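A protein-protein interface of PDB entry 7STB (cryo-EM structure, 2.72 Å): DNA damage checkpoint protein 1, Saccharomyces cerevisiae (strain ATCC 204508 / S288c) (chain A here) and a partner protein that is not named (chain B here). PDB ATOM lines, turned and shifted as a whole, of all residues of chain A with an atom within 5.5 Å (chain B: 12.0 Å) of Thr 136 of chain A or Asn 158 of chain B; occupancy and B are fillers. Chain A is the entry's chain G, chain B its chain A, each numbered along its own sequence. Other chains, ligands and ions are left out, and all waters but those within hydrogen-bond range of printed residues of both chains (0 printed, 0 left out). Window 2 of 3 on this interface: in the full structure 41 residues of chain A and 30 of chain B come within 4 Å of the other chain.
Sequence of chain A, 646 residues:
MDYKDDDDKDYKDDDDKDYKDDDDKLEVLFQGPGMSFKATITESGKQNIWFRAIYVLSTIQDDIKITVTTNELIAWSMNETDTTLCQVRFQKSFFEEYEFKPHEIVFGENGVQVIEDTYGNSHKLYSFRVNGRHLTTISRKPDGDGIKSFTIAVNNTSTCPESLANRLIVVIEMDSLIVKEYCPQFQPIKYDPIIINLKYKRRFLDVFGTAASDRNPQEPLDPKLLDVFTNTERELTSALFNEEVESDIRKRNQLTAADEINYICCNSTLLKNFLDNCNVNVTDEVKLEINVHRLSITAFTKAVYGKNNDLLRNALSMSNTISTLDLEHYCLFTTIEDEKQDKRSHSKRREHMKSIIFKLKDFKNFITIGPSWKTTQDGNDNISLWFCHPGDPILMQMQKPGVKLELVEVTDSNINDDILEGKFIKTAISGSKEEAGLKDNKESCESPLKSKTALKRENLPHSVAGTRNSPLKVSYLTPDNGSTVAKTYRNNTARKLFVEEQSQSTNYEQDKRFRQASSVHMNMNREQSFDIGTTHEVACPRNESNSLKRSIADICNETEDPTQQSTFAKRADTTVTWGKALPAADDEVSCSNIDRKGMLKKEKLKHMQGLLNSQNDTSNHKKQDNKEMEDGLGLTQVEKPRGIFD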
ATOM      1  N   PHE A  51     -31.620  -5.879 -16.339  1.00  0.00           N
ATOM      2  CA  PHE A  51     -30.546  -6.778 -15.942  1.00  0.00           C
ATOM      3  C   PHE A  51     -29.246  -6.016 -15.729  1.00  0.00           C
ATOM      4  O   PHE A  51     -28.512  -6.284 -14.771  1.00  0.00           O
ATOM      5  CB  PHE A  51     -30.356  -7.872 -16.992  1.00  0.00           C
ATOM      6  CG  PHE A  51     -29.032  -8.573 -16.899  1.00  0.00           C
ATOM      7  CD1 PHE A  51     -28.793  -9.499 -15.899  1.00  0.00           C
ATOM      8  CD2 PHE A  51     -28.023  -8.302 -17.806  1.00  0.00           C
ATOM      9  CE1 PHE A  51     -27.576 -10.142 -15.808  1.00  0.00           C
ATOM     10  CE2 PHE A  51     -26.804  -8.942 -17.720  1.00  0.00           C
ATOM     11  CZ  PHE A  51     -26.580  -9.863 -16.719  1.00  0.00           C
ATOM     12  N   ILE A  54     -29.437  -4.072 -12.429  1.00  0.00           N
ATOM     13  CA  ILE A  54     -29.311  -4.966 -11.282  1.00  0.00           C
ATOM     14  C   ILE A  54     -27.871  -5.438 -11.132  1.00  0.00           C
ATOM     15  O   ILE A  54     -27.343  -5.525 -10.018  1.00  0.00           O
ATOM     16  CB  ILE A  54     -30.289  -6.149 -11.414  1.00  0.00           C
ATOM     17  CG1 ILE A  54     -31.740  -5.658 -11.369  1.00  0.00           C
ATOM     18  CG2 ILE A  54     -30.042  -7.173 -10.316  1.00  0.00           C
ATOM     19  CD1 ILE A  54     -32.127  -4.932 -10.093  1.00  0.00           C
ATOM     20  N   TYR A  55     -27.210  -5.750 -12.250  1.00  0.00           N
ATOM     21  CA  TYR A  55     -25.817  -6.182 -12.187  1.00  0.00           C
ATOM     22  C   TYR A  55     -24.926  -5.081 -11.628  1.00  0.00           C
ATOM     23  O   TYR A  55     -24.060  -5.339 -10.784  1.00  0.00           O
ATOM     24  CB  TYR A  55     -25.341  -6.610 -13.576  1.00  0.00           C
ATOM     25  CG  TYR A  55     -23.875  -6.980 -13.634  1.00  0.00           C
ATOM     26  CD1 TYR A  55     -23.434  -8.212 -13.175  1.00  0.00           C
ATOM     27  CD2 TYR A  55     -22.934  -6.096 -14.145  1.00  0.00           C
ATOM     28  CE1 TYR A  55     -22.098  -8.554 -13.222  1.00  0.00           C
ATOM     29  CE2 TYR A  55     -21.596  -6.430 -14.195  1.00  0.00           C
ATOM     30  CZ  TYR A  55     -21.184  -7.660 -13.733  1.00  0.00           C
ATOM     31  OH  TYR A  55     -19.852  -8.002 -13.781  1.00  0.00           O
ATOM     32  N   SER A  58     -25.531  -4.728  -7.897  1.00  0.00           N
ATOM     33  CA  SER A  58     -24.845  -5.813  -7.208  1.00  0.00           C
ATOM     34  C   SER A  58     -23.338  -5.597  -7.202  1.00  0.00           C
ATOM     35  O   SER A  58     -22.641  -6.101  -6.315  1.00  0.00           O
ATOM     36  CB  SER A  58     -25.189  -7.153  -7.862  1.00  0.00           C
ATOM     37  OG  SER A  58     -24.568  -7.281  -9.126  1.00  0.00           O
ATOM     38  N   THR A  59     -22.815  -4.867  -8.189  1.00  0.00           N
ATOM     39  CA  THR A  59     -21.393  -4.534  -8.174  1.00  0.00           C
ATOM     40  C   THR A  59     -21.064  -3.562  -7.046  1.00  0.00           C
ATOM     41  O   THR A  59     -20.055  -3.733  -6.351  1.00  0.00           O
ATOM     42  CB  THR A  59     -20.963  -3.949  -9.519  1.00  0.00           C
ATOM     43  OG1 THR A  59     -21.698  -2.748  -9.784  1.00  0.00           O
ATOM     44  CG2 THR A  59     -21.194  -4.948 -10.642  1.00  0.00           C
ATOM     45  N   ILE A  64     -28.788  -5.486  -2.578  1.00  0.00           N
ATOM     46  CA  ILE A  64     -29.463  -4.367  -3.222  1.00  0.00           C
ATOM     47  C   ILE A  64     -30.724  -4.046  -2.435  1.00  0.00           C
ATOM     48  O   ILE A  64     -31.399  -4.948  -1.919  1.00  0.00           O
ATOM     49  CB  ILE A  64     -29.796  -4.699  -4.689  1.00  0.00           C
ATOM     50  CG1 ILE A  64     -28.515  -4.980  -5.479  1.00  0.00           C
ATOM     51  CG2 ILE A  64     -30.578  -3.562  -5.332  1.00  0.00           C
ATOM     52  CD1 ILE A  64     -28.762  -5.654  -6.811  1.00  0.00           C
ATOM     53  N   ASN A 131     -30.399 -10.141  -1.864  1.00  0.00           N
ATOM     54  CA  ASN A 131     -29.068 -10.457  -2.364  1.00  0.00           C
ATOM     55  C   ASN A 131     -28.961 -10.076  -3.837  1.00  0.00           C
ATOM     56  O   ASN A 131     -29.727 -10.567  -4.673  1.00  0.00           O
ATOM     57  CB  ASN A 131     -28.777 -11.942  -2.168  1.00  0.00           C
ATOM     58  CG  ASN A 131     -27.394 -12.333  -2.643  1.00  0.00           C
ATOM     59  OD1 ASN A 131     -27.067 -12.193  -3.818  1.00  0.00           O
ATOM     60  ND2 ASN A 131     -26.573 -12.825  -1.726  1.00  0.00           N
ATOM     61  N   GLY A 132     -28.010  -9.195  -4.151  1.00  0.00           N
ATOM     62  CA  GLY A 132     -27.879  -8.715  -5.517  1.00  0.00           C
ATOM     63  C   GLY A 132     -27.443  -9.796  -6.487  1.00  0.00           C
ATOM     64  O   GLY A 132     -27.904  -9.836  -7.630  1.00  0.00           O
ATOM     65  N   ARG A 133     -26.542 -10.680  -6.052  1.00  0.00           N
ATOM     66  CA  ARG A 133     -26.058 -11.732  -6.939  1.00  0.00           C
ATOM     67  C   ARG A 133     -27.195 -12.645  -7.383  1.00  0.00           C
ATOM     68  O   ARG A 133     -27.277 -13.018  -8.558  1.00  0.00           O
ATOM     69  CB  ARG A 133     -24.962 -12.540  -6.245  1.00  0.00           C
ATOM     70  CG  ARG A 133     -23.674 -11.768  -6.028  1.00  0.00           C
ATOM     71  CD  ARG A 133     -22.516 -12.692  -5.692  1.00  0.00           C
ATOM     72  NE  ARG A 133     -22.936 -13.833  -4.888  1.00  0.00           N
ATOM     73  CZ  ARG A 133     -23.104 -13.807  -3.572  1.00  0.00           C
ATOM     74  NH1 ARG A 133     -22.899 -12.703  -2.870  1.00  0.00           N
ATOM     75  NH2 ARG A 133     -23.488 -14.914  -2.945  1.00  0.00           N
ATOM     76  N   HIS A 134     -28.077 -13.023  -6.455  1.00  0.00           N
ATOM     77  CA  HIS A 134     -29.199 -13.883  -6.816  1.00  0.00           C
ATOM     78  C   HIS A 134     -30.140 -13.191  -7.794  1.00  0.00           C
ATOM     79  O   HIS A 134     -30.595 -13.803  -8.767  1.00  0.00           O
ATOM     80  CB  HIS A 134     -29.957 -14.315  -5.561  1.00  0.00           C
ATOM     81  CG  HIS A 134     -29.127 -15.099  -4.593  1.00  0.00           C
ATOM     82  ND1 HIS A 134     -29.338 -15.065  -3.232  1.00  0.00           N
ATOM     83  CD2 HIS A 134     -28.079 -15.933  -4.790  1.00  0.00           C
ATOM     84  CE1 HIS A 134     -28.461 -15.850  -2.633  1.00  0.00           C
ATOM     85  NE2 HIS A 134     -27.684 -16.387  -3.556  1.00  0.00           N
ATOM     86  N   LEU A 135     -30.446 -11.916  -7.556  1.00  0.00           N
ATOM     87  CA  LEU A 135     -31.326 -11.198  -8.472  1.00  0.00           C
ATOM     88  C   LEU A 135     -30.702 -11.099  -9.857  1.00  0.00           C
ATOM     89  O   LEU A 135     -31.392 -11.253 -10.872  1.00  0.00           O
ATOM     90  CB  LEU A 135     -31.641  -9.809  -7.915  1.00  0.00           C
ATOM     91  CG  LEU A 135     -32.830  -9.072  -8.538  1.00  0.00           C
ATOM     92  CD1 LEU A 135     -34.104  -9.900  -8.458  1.00  0.00           C
ATOM     93  CD2 LEU A 135     -33.029  -7.725  -7.864  1.00  0.00           C
ATOM     94  N   THR A 136     -29.394 -10.843  -9.920  1.00  0.00           N
ATOM     95  CA  THR A 136     -28.716 -10.785 -11.211  1.00  0.00           C
ATOM     96  C   THR A 136     -28.755 -12.135 -11.915  1.00  0.00           C
ATOM     97  O   THR A 136     -29.028 -12.207 -13.119  1.00  0.00           O
ATOM     98  CB  THR A 136     -27.271 -10.322 -11.020  1.00  0.00           C
ATOM     99  OG1 THR A 136     -27.255  -9.076 -10.317  1.00  0.00           O
ATOM    100  CG2 THR A 136     -26.582 -10.149 -12.364  1.00  0.00           C
ATOM    101  N   THR A 137     -28.487 -13.219 -11.182  1.00  0.00           N
ATOM    102  CA  THR A 137     -28.527 -14.552 -11.775  1.00  0.00           C
ATOM    103  C   THR A 137     -29.943 -14.981 -12.134  1.00  0.00           C
ATOM    104  O   THR A 137     -30.113 -15.957 -12.870  1.00  0.00           O
ATOM    105  CB  THR A 137     -27.907 -15.574 -10.820  1.00  0.00           C
ATOM    106  OG1 THR A 137     -26.647 -15.087 -10.344  1.00  0.00           O
ATOM    107  CG2 THR A 137     -27.697 -16.908 -11.522  1.00  0.00           C
ATOM    108  N   ILE A 138     -30.955 -14.298 -11.609  1.00  0.00           N
ATOM    109  CA  ILE A 138     -32.328 -14.576 -12.012  1.00  0.00           C
ATOM    110  C   ILE A 138     -32.748 -13.726 -13.210  1.00  0.00           C
ATOM    111  O   ILE A 138     -33.609 -14.145 -13.991  1.00  0.00           O
ATOM    112  CB  ILE A 138     -33.281 -14.361 -10.824  1.00  0.00           C
ATOM    113  CG1 ILE A 138     -33.125 -15.494  -9.809  1.00  0.00           C
ATOM    114  CG2 ILE A 138     -34.725 -14.272 -11.304  1.00  0.00           C
ATOM    115  CD1 ILE A 138     -33.826 -15.239  -8.491  1.00  0.00           C
ATOM    116  N   SER A 139     -32.162 -12.540 -13.373  1.00  0.00           N
ATOM    117  CA  SER A 139     -32.577 -11.613 -14.417  1.00  0.00           C
ATOM    118  C   SER A 139     -31.788 -11.754 -15.713  1.00  0.00           C
ATOM    119  O   SER A 139     -32.121 -11.080 -16.693  1.00  0.00           O
ATOM    120  CB  SER A 139     -32.450 -10.170 -13.913  1.00  0.00           C
ATOM    121  OG  SER A 139     -33.237  -9.963 -12.755  1.00  0.00           O
ATOM    122  N   ARG A 140     -30.762 -12.601 -15.753  1.00  0.00           N
ATOM    123  CA  ARG A 140     -29.936 -12.703 -16.949  1.00  0.00           C
ATOM    124  C   ARG A 140     -30.719 -13.331 -18.098  1.00  0.00           C
ATOM    125  O   ARG A 140     -31.584 -14.189 -17.900  1.00  0.00           O
ATOM    126  CB  ARG A 140     -28.670 -13.515 -16.664  1.00  0.00           C
ATOM    127  CG  ARG A 140     -28.815 -15.026 -16.811  1.00  0.00           C
ATOM    128  CD  ARG A 140     -29.798 -15.582 -15.804  1.00  0.00           C
ATOM    129  NE  ARG A 140     -29.853 -17.040 -15.824  1.00  0.00           N
ATOM    130  CZ  ARG A 140     -30.611 -17.753 -16.646  1.00  0.00           C
ATOM    131  NH1 ARG A 140     -31.394 -17.176 -17.542  1.00  0.00           N
ATOM    132  NH2 ARG A 140     -30.583 -19.080 -16.566  1.00  0.00           N
ATOM    133  N   ARG B 152     -16.004  -4.978   6.425  1.00  0.00           N
ATOM    134  CA  ARG B 152     -16.734  -6.231   6.573  1.00  0.00           C
ATOM    135  C   ARG B 152     -16.086  -7.284   5.682  1.00  0.00           C
ATOM    136  O   ARG B 152     -16.012  -7.109   4.461  1.00  0.00           O
ATOM    137  CB  ARG B 152     -18.208  -6.045   6.216  1.00  0.00           C
ATOM    138  CG  ARG B 152     -19.096  -7.194   6.653  1.00  0.00           C
ATOM    139  CD  ARG B 152     -20.555  -6.772   6.743  1.00  0.00           C
ATOM    140  NE  ARG B 152     -20.989  -6.023   5.569  1.00  0.00           N
ATOM    141  CZ  ARG B 152     -21.178  -6.552   4.369  1.00  0.00           C
ATOM    142  NH1 ARG B 152     -20.987  -7.841   4.141  1.00  0.00           N
ATOM    143  NH2 ARG B 152     -21.573  -5.767   3.370  1.00  0.00           N
ATOM    144  N   ASP B 154     -17.009 -10.413   4.984  1.00  0.00           N
ATOM    145  CA  ASP B 154     -17.874 -11.352   4.281  1.00  0.00           C
ATOM    146  C   ASP B 154     -18.689 -10.686   3.180  1.00  0.00           C
ATOM    147  O   ASP B 154     -19.690 -11.257   2.732  1.00  0.00           O
ATOM    148  CB  ASP B 154     -18.797 -12.069   5.273  1.00  0.00           C
ATOM    149  CG  ASP B 154     -19.870 -11.160   5.851  1.00  0.00           C
ATOM    150  OD1 ASP B 154     -19.948  -9.978   5.461  1.00  0.00           O
ATOM    151  OD2 ASP B 154     -20.645 -11.638   6.705  1.00  0.00           O
ATOM    152  N   CYS B 155     -18.292  -9.498   2.735  1.00  0.00           N
ATOM    153  CA  CYS B 155     -18.977  -8.821   1.642  1.00  0.00           C
ATOM    154  C   CYS B 155     -18.489  -9.392   0.317  1.00  0.00           C
ATOM    155  O   CYS B 155     -17.282  -9.431   0.058  1.00  0.00           O
ATOM    156  CB  CYS B 155     -18.727  -7.316   1.705  1.00  0.00           C
ATOM    157  SG  CYS B 155     -19.677  -6.356   0.504  1.00  0.00           S
ATOM    158  N   ILE B 156     -19.422  -9.836  -0.517  1.00  0.00           N
ATOM    159  CA  ILE B 156     -19.110 -10.431  -1.814  1.00  0.00           C
ATOM    160  C   ILE B 156     -19.894  -9.645  -2.857  1.00  0.00           C
ATOM    161  O   ILE B 156     -21.061  -9.934  -3.132  1.00  0.00           O
ATOM    162  CB  ILE B 156     -19.448 -11.924  -1.872  1.00  0.00           C
ATOM    163  CG1 ILE B 156     -18.604 -12.708  -0.865  1.00  0.00           C
ATOM    164  CG2 ILE B 156     -19.219 -12.466  -3.276  1.00  0.00           C
ATOM    165  CD1 ILE B 156     -19.214 -14.037  -0.475  1.00  0.00           C
ATOM    166  N   VAL B 157     -19.254  -8.637  -3.449  1.00  0.00           N
ATOM    167  CA  VAL B 157     -19.866  -7.923  -4.561  1.00  0.00           C
ATOM    168  C   VAL B 157     -19.705  -8.742  -5.838  1.00  0.00           C
ATOM    169  O   VAL B 157     -18.907  -9.679  -5.917  1.00  0.00           O
ATOM    170  CB  VAL B 157     -19.271  -6.512  -4.722  1.00  0.00           C
ATOM    171  CG1 VAL B 157     -19.696  -5.624  -3.564  1.00  0.00           C
ATOM    172  CG2 VAL B 157     -17.757  -6.570  -4.832  1.00  0.00           C
ATOM    173  N   ASN B 158     -20.478  -8.374  -6.860  1.00  0.00           N
ATOM    174  CA  ASN B 158     -20.554  -9.200  -8.061  1.00  0.00           C
ATOM    175  C   ASN B 158     -19.260  -9.132  -8.866  1.00  0.00           C
ATOM    176  O   ASN B 158     -18.589 -10.149  -9.072  1.00  0.00           O
ATOM    177  CB  ASN B 158     -21.749  -8.765  -8.912  1.00  0.00           C
ATOM    178  CG  ASN B 158     -22.403  -9.926  -9.633  1.00  0.00           C
ATOM    179  OD1 ASN B 158     -21.901 -11.049  -9.610  1.00  0.00           O
ATOM    180  ND2 ASN B 158     -23.535  -9.661 -10.272  1.00  0.00           N
ATOM    181  N   ASP B 159     -18.893  -7.939  -9.328  1.00  0.00           N
ATOM    182  CA  ASP B 159     -17.740  -7.773 -10.213  1.00  0.00           C
ATOM    183  C   ASP B 159     -16.512  -7.362  -9.401  1.00  0.00           C
ATOM    184  O   ASP B 159     -16.035  -6.228  -9.459  1.00  0.00           O
ATOM    185  CB  ASP B 159     -18.055  -6.752 -11.301  1.00  0.00           C
ATOM    186  CG  ASP B 159     -16.926  -6.594 -12.298  1.00  0.00           C
ATOM    187  OD1 ASP B 159     -16.001  -7.433 -12.290  1.00  0.00           O
ATOM    188  OD2 ASP B 159     -16.962  -5.628 -13.090  1.00  0.00           O
ATOM    189  N   LEU B 160     -15.996  -8.319  -8.632  1.00  0.00           N
ATOM    190  CA  LEU B 160     -14.783  -8.074  -7.864  1.00  0.00           C
ATOM    191  C   LEU B 160     -14.177  -9.380  -7.363  1.00  0.00           C
ATOM    192  O   LEU B 160     -14.878 -10.190  -6.745  1.00  0.00           O
ATOM    193  CB  LEU B 160     -15.076  -7.154  -6.678  1.00  0.00           C
ATOM    194  CG  LEU B 160     -13.866  -6.433  -6.086  1.00  0.00           C
ATOM    195  CD1 LEU B 160     -13.440  -5.273  -6.974  1.00  0.00           C
ATOM    196  CD2 LEU B 160     -14.171  -5.953  -4.678  1.00  0.00           C
ATOM    197  N   PRO B 161     -12.889  -9.625  -7.601  1.00  0.00           N
ATOM    198  CA  PRO B 161     -12.230 -10.760  -6.948  1.00  0.00           C
ATOM    199  C   PRO B 161     -12.158 -10.562  -5.443  1.00  0.00           C
ATOM    200  O   PRO B 161     -12.118  -9.436  -4.940  1.00  0.00           O
ATOM    201  CB  PRO B 161     -10.832 -10.779  -7.580  1.00  0.00           C
ATOM    202  CG  PRO B 161     -10.964 -10.007  -8.842  1.00  0.00           C
ATOM    203  CD  PRO B 161     -12.009  -8.975  -8.587  1.00  0.00           C
ATOM    204  N   GLN B 162     -12.142 -11.683  -4.718  1.00  0.00           N
ATOM    205  CA  GLN B 162     -12.194 -11.623  -3.261  1.00  0.00           C
ATOM    206  C   GLN B 162     -10.995 -10.873  -2.692  1.00  0.00           C
ATOM    207  O   GLN B 162     -11.148  -9.988  -1.841  1.00  0.00           O
ATOM    208  CB  GLN B 162     -12.268 -13.036  -2.684  1.00  0.00           C
ATOM    209  CG  GLN B 162     -12.792 -13.096  -1.257  1.00  0.00           C
ATOM    210  CD  GLN B 162     -14.276 -12.796  -1.167  1.00  0.00           C
ATOM    211  OE1 GLN B 162     -15.106 -13.556  -1.664  1.00  0.00           O
ATOM    212  NE2 GLN B 162     -14.616 -11.682  -0.529  1.00  0.00           N
ATOM    213  N   MET B 163      -9.787 -11.202  -3.160  1.00  0.00           N
ATOM    214  CA  MET B 163      -8.589 -10.581  -2.603  1.00  0.00           C
ATOM    215  C   MET B 163      -8.573  -9.073  -2.803  1.00  0.00           C
ATOM    216  O   MET B 163      -7.876  -8.369  -2.064  1.00  0.00           O
ATOM    217  CB  MET B 163      -7.329 -11.184  -3.225  1.00  0.00           C
ATOM    218  CG  MET B 163      -7.097 -12.639  -2.875  1.00  0.00           C
ATOM    219  SD  MET B 163      -5.564 -13.278  -3.575  1.00  0.00           S
ATOM    220  CE  MET B 163      -6.015 -13.432  -5.297  1.00  0.00           C
ATOM    221  N   GLU B 164      -9.315  -8.561  -3.779  1.00  0.00           N
ATOM    222  CA  GLU B 164      -9.362  -7.132  -4.046  1.00  0.00           C
ATOM    223  C   GLU B 164     -10.403  -6.407  -3.204  1.00  0.00           C
ATOM    224  O   GLU B 164     -10.547  -5.189  -3.342  1.00  0.00           O
ATOM    225  CB  GLU B 164      -9.645  -6.883  -5.532  1.00  0.00           C
ATOM    226  CG  GLU B 164      -8.566  -7.409  -6.467  1.00  0.00           C
ATOM    227  CD  GLU B 164      -7.201  -6.811  -6.181  1.00  0.00           C
ATOM    228  OE1 GLU B 164      -7.104  -5.571  -6.074  1.00  0.00           O
ATOM    229  OE2 GLU B 164      -6.226  -7.581  -6.063  1.00  0.00           O
ATOM    230  N   SER B 165     -11.131  -7.117  -2.340  1.00  0.00           N
ATOM    231  CA  SER B 165     -12.164  -6.465  -1.543  1.00  0.00           C
ATOM    232  C   SER B 165     -11.562  -5.408  -0.624  1.00  0.00           C
ATOM    233  O   SER B 165     -11.953  -4.235  -0.667  1.00  0.00           O
ATOM    234  CB  SER B 165     -12.931  -7.509  -0.732  1.00  0.00           C
ATOM    235  OG  SER B 165     -14.095  -6.950  -0.149  1.00  0.00           O
ATOM    236  N   GLU B 168     -10.447  -2.297  -2.299  1.00  0.00           N
ATOM    237  CA  GLU B 168     -11.561  -1.425  -2.653  1.00  0.00           C
ATOM    238  C   GLU B 168     -12.077  -0.669  -1.440  1.00  0.00           C
ATOM    239  O   GLU B 168     -12.557   0.463  -1.571  1.00  0.00           O
ATOM    240  CB  GLU B 168     -12.688  -2.236  -3.293  1.00  0.00           C
ATOM    241  CG  GLU B 168     -12.321  -2.839  -4.638  1.00  0.00           C
ATOM    242  CD  GLU B 168     -12.095  -1.790  -5.708  1.00  0.00           C
ATOM    243  OE1 GLU B 168     -12.750  -0.729  -5.651  1.00  0.00           O
ATOM    244  OE2 GLU B 168     -11.257  -2.025  -6.604  1.00  0.00           O
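O of Arg 133 of chain A sits at hydrogen-bond distance from OG1 of Thr 137 of chain A, 2.8 Å away.
The backbone carbonyl oxygen (O) of Ile 54 of chain A sits at hydrogen-bond distance from the side-chain hydroxyl (OG) of Ser 58 of chain A (3.4 Å).
OG of Ser 58 of chain A lies within hydrogen-bond range of O of Tyr 55 of chain A (2.6 Å).
OD1 of Asn 131 of chain A sits at hydrogen-bond distance from N of Arg 133 of chain A (2.7 Å).
OG1 of Thr 136 of chain A sits at hydrogen-bond distance from O of Gly 132 of chain A (2.9 Å).
The side-chain hydroxyl of Ser 58 of chain A lies within hydrogen-bond range of the side-chain hydroxyl of Thr 136 of chain A (3.4 Å).
Asn 158 of chain B touches three residues of chain A.
No residue of chain B comes within 4 Å of Phe 51 of chain A.
Of chain B, only Asn 158 and Asp 159 come within 4 Å of Tyr 55 of chain A.
Ser 58 of chain A touches just these residues of chain B: Val 157 (3.8 Å) and Asn 158 (2.8 Å).
Of chain B, only Val 157 (3.3 Å) and Asp 159 (3.7 Å) come within 4 Å of Thr 59 of chain A.
No residue of chain B comes within 4 Å of Gly 132 of chain A.
No residue of chain B comes within 4 Å of Leu 135 of chain A.
No residue of chain B comes within 4 Å of Thr 137 of chain A.
No residue of chain B comes within 4 Å of Ser 139 of chain A.
Arg 140 of chain A touches none of the printed residues of chain B.
Of the printed residues of chain A, Val 157 of chain B touches Ser 58 and Thr 59.
Printed residues of chain A within 4 Å of Asp 159 of chain B: Tyr 55 (3.3 Å) and Thr 59 (3.7 Å).
Of the printed residues of chain A, Ile 156 of chain B touches Arg 133.
Met 163 of chain B touches none of the printed residues of chain A.
The nearest printed residue of chain A that does not touch Asp 159 of chain B is Ser 58 of chain A (5.1 Å).
Printed residues of chain A that touch a printed residue of chain B: Tyr 55, Ser 58, Thr 59, Arg 133 and Thr 136.
Along chain A the printed residues that touch a printed residue of chain B span positions 55 to 136.
Among the printed residues, 8 pairs touch across the chains.
Among the printed residues, no Asp or Glu carboxylate lies within 4 Å of a Lys or Arg side-chain nitrogen of the other chain.
Asn 158 of chain B touches Tyr 55 of chain A (ND2 to CD1, 3.2 Å).
Asp 159 of chain B touches Tyr 55 of chain A.
Val 157 of chain B touches Ser 58 of chain A.
Thr 59 of chain A touches Val 157 of chain B.
Asp 159 of chain B touches Thr 59 of chain A (CB to CG2, 3.7 Å).
CG2 of Thr 136 of chain A touches ND2 of Asn 158 of chain B (3.7 Å).
ND2 of Asn 158 of chain B lies within hydrogen-bond range of OG of Ser 58 of chain A (2.8 Å).
O of Ile 156 of chain B is in hydrogen-bond range of NH1 of Arg 133 of chain A (3.3 Å).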
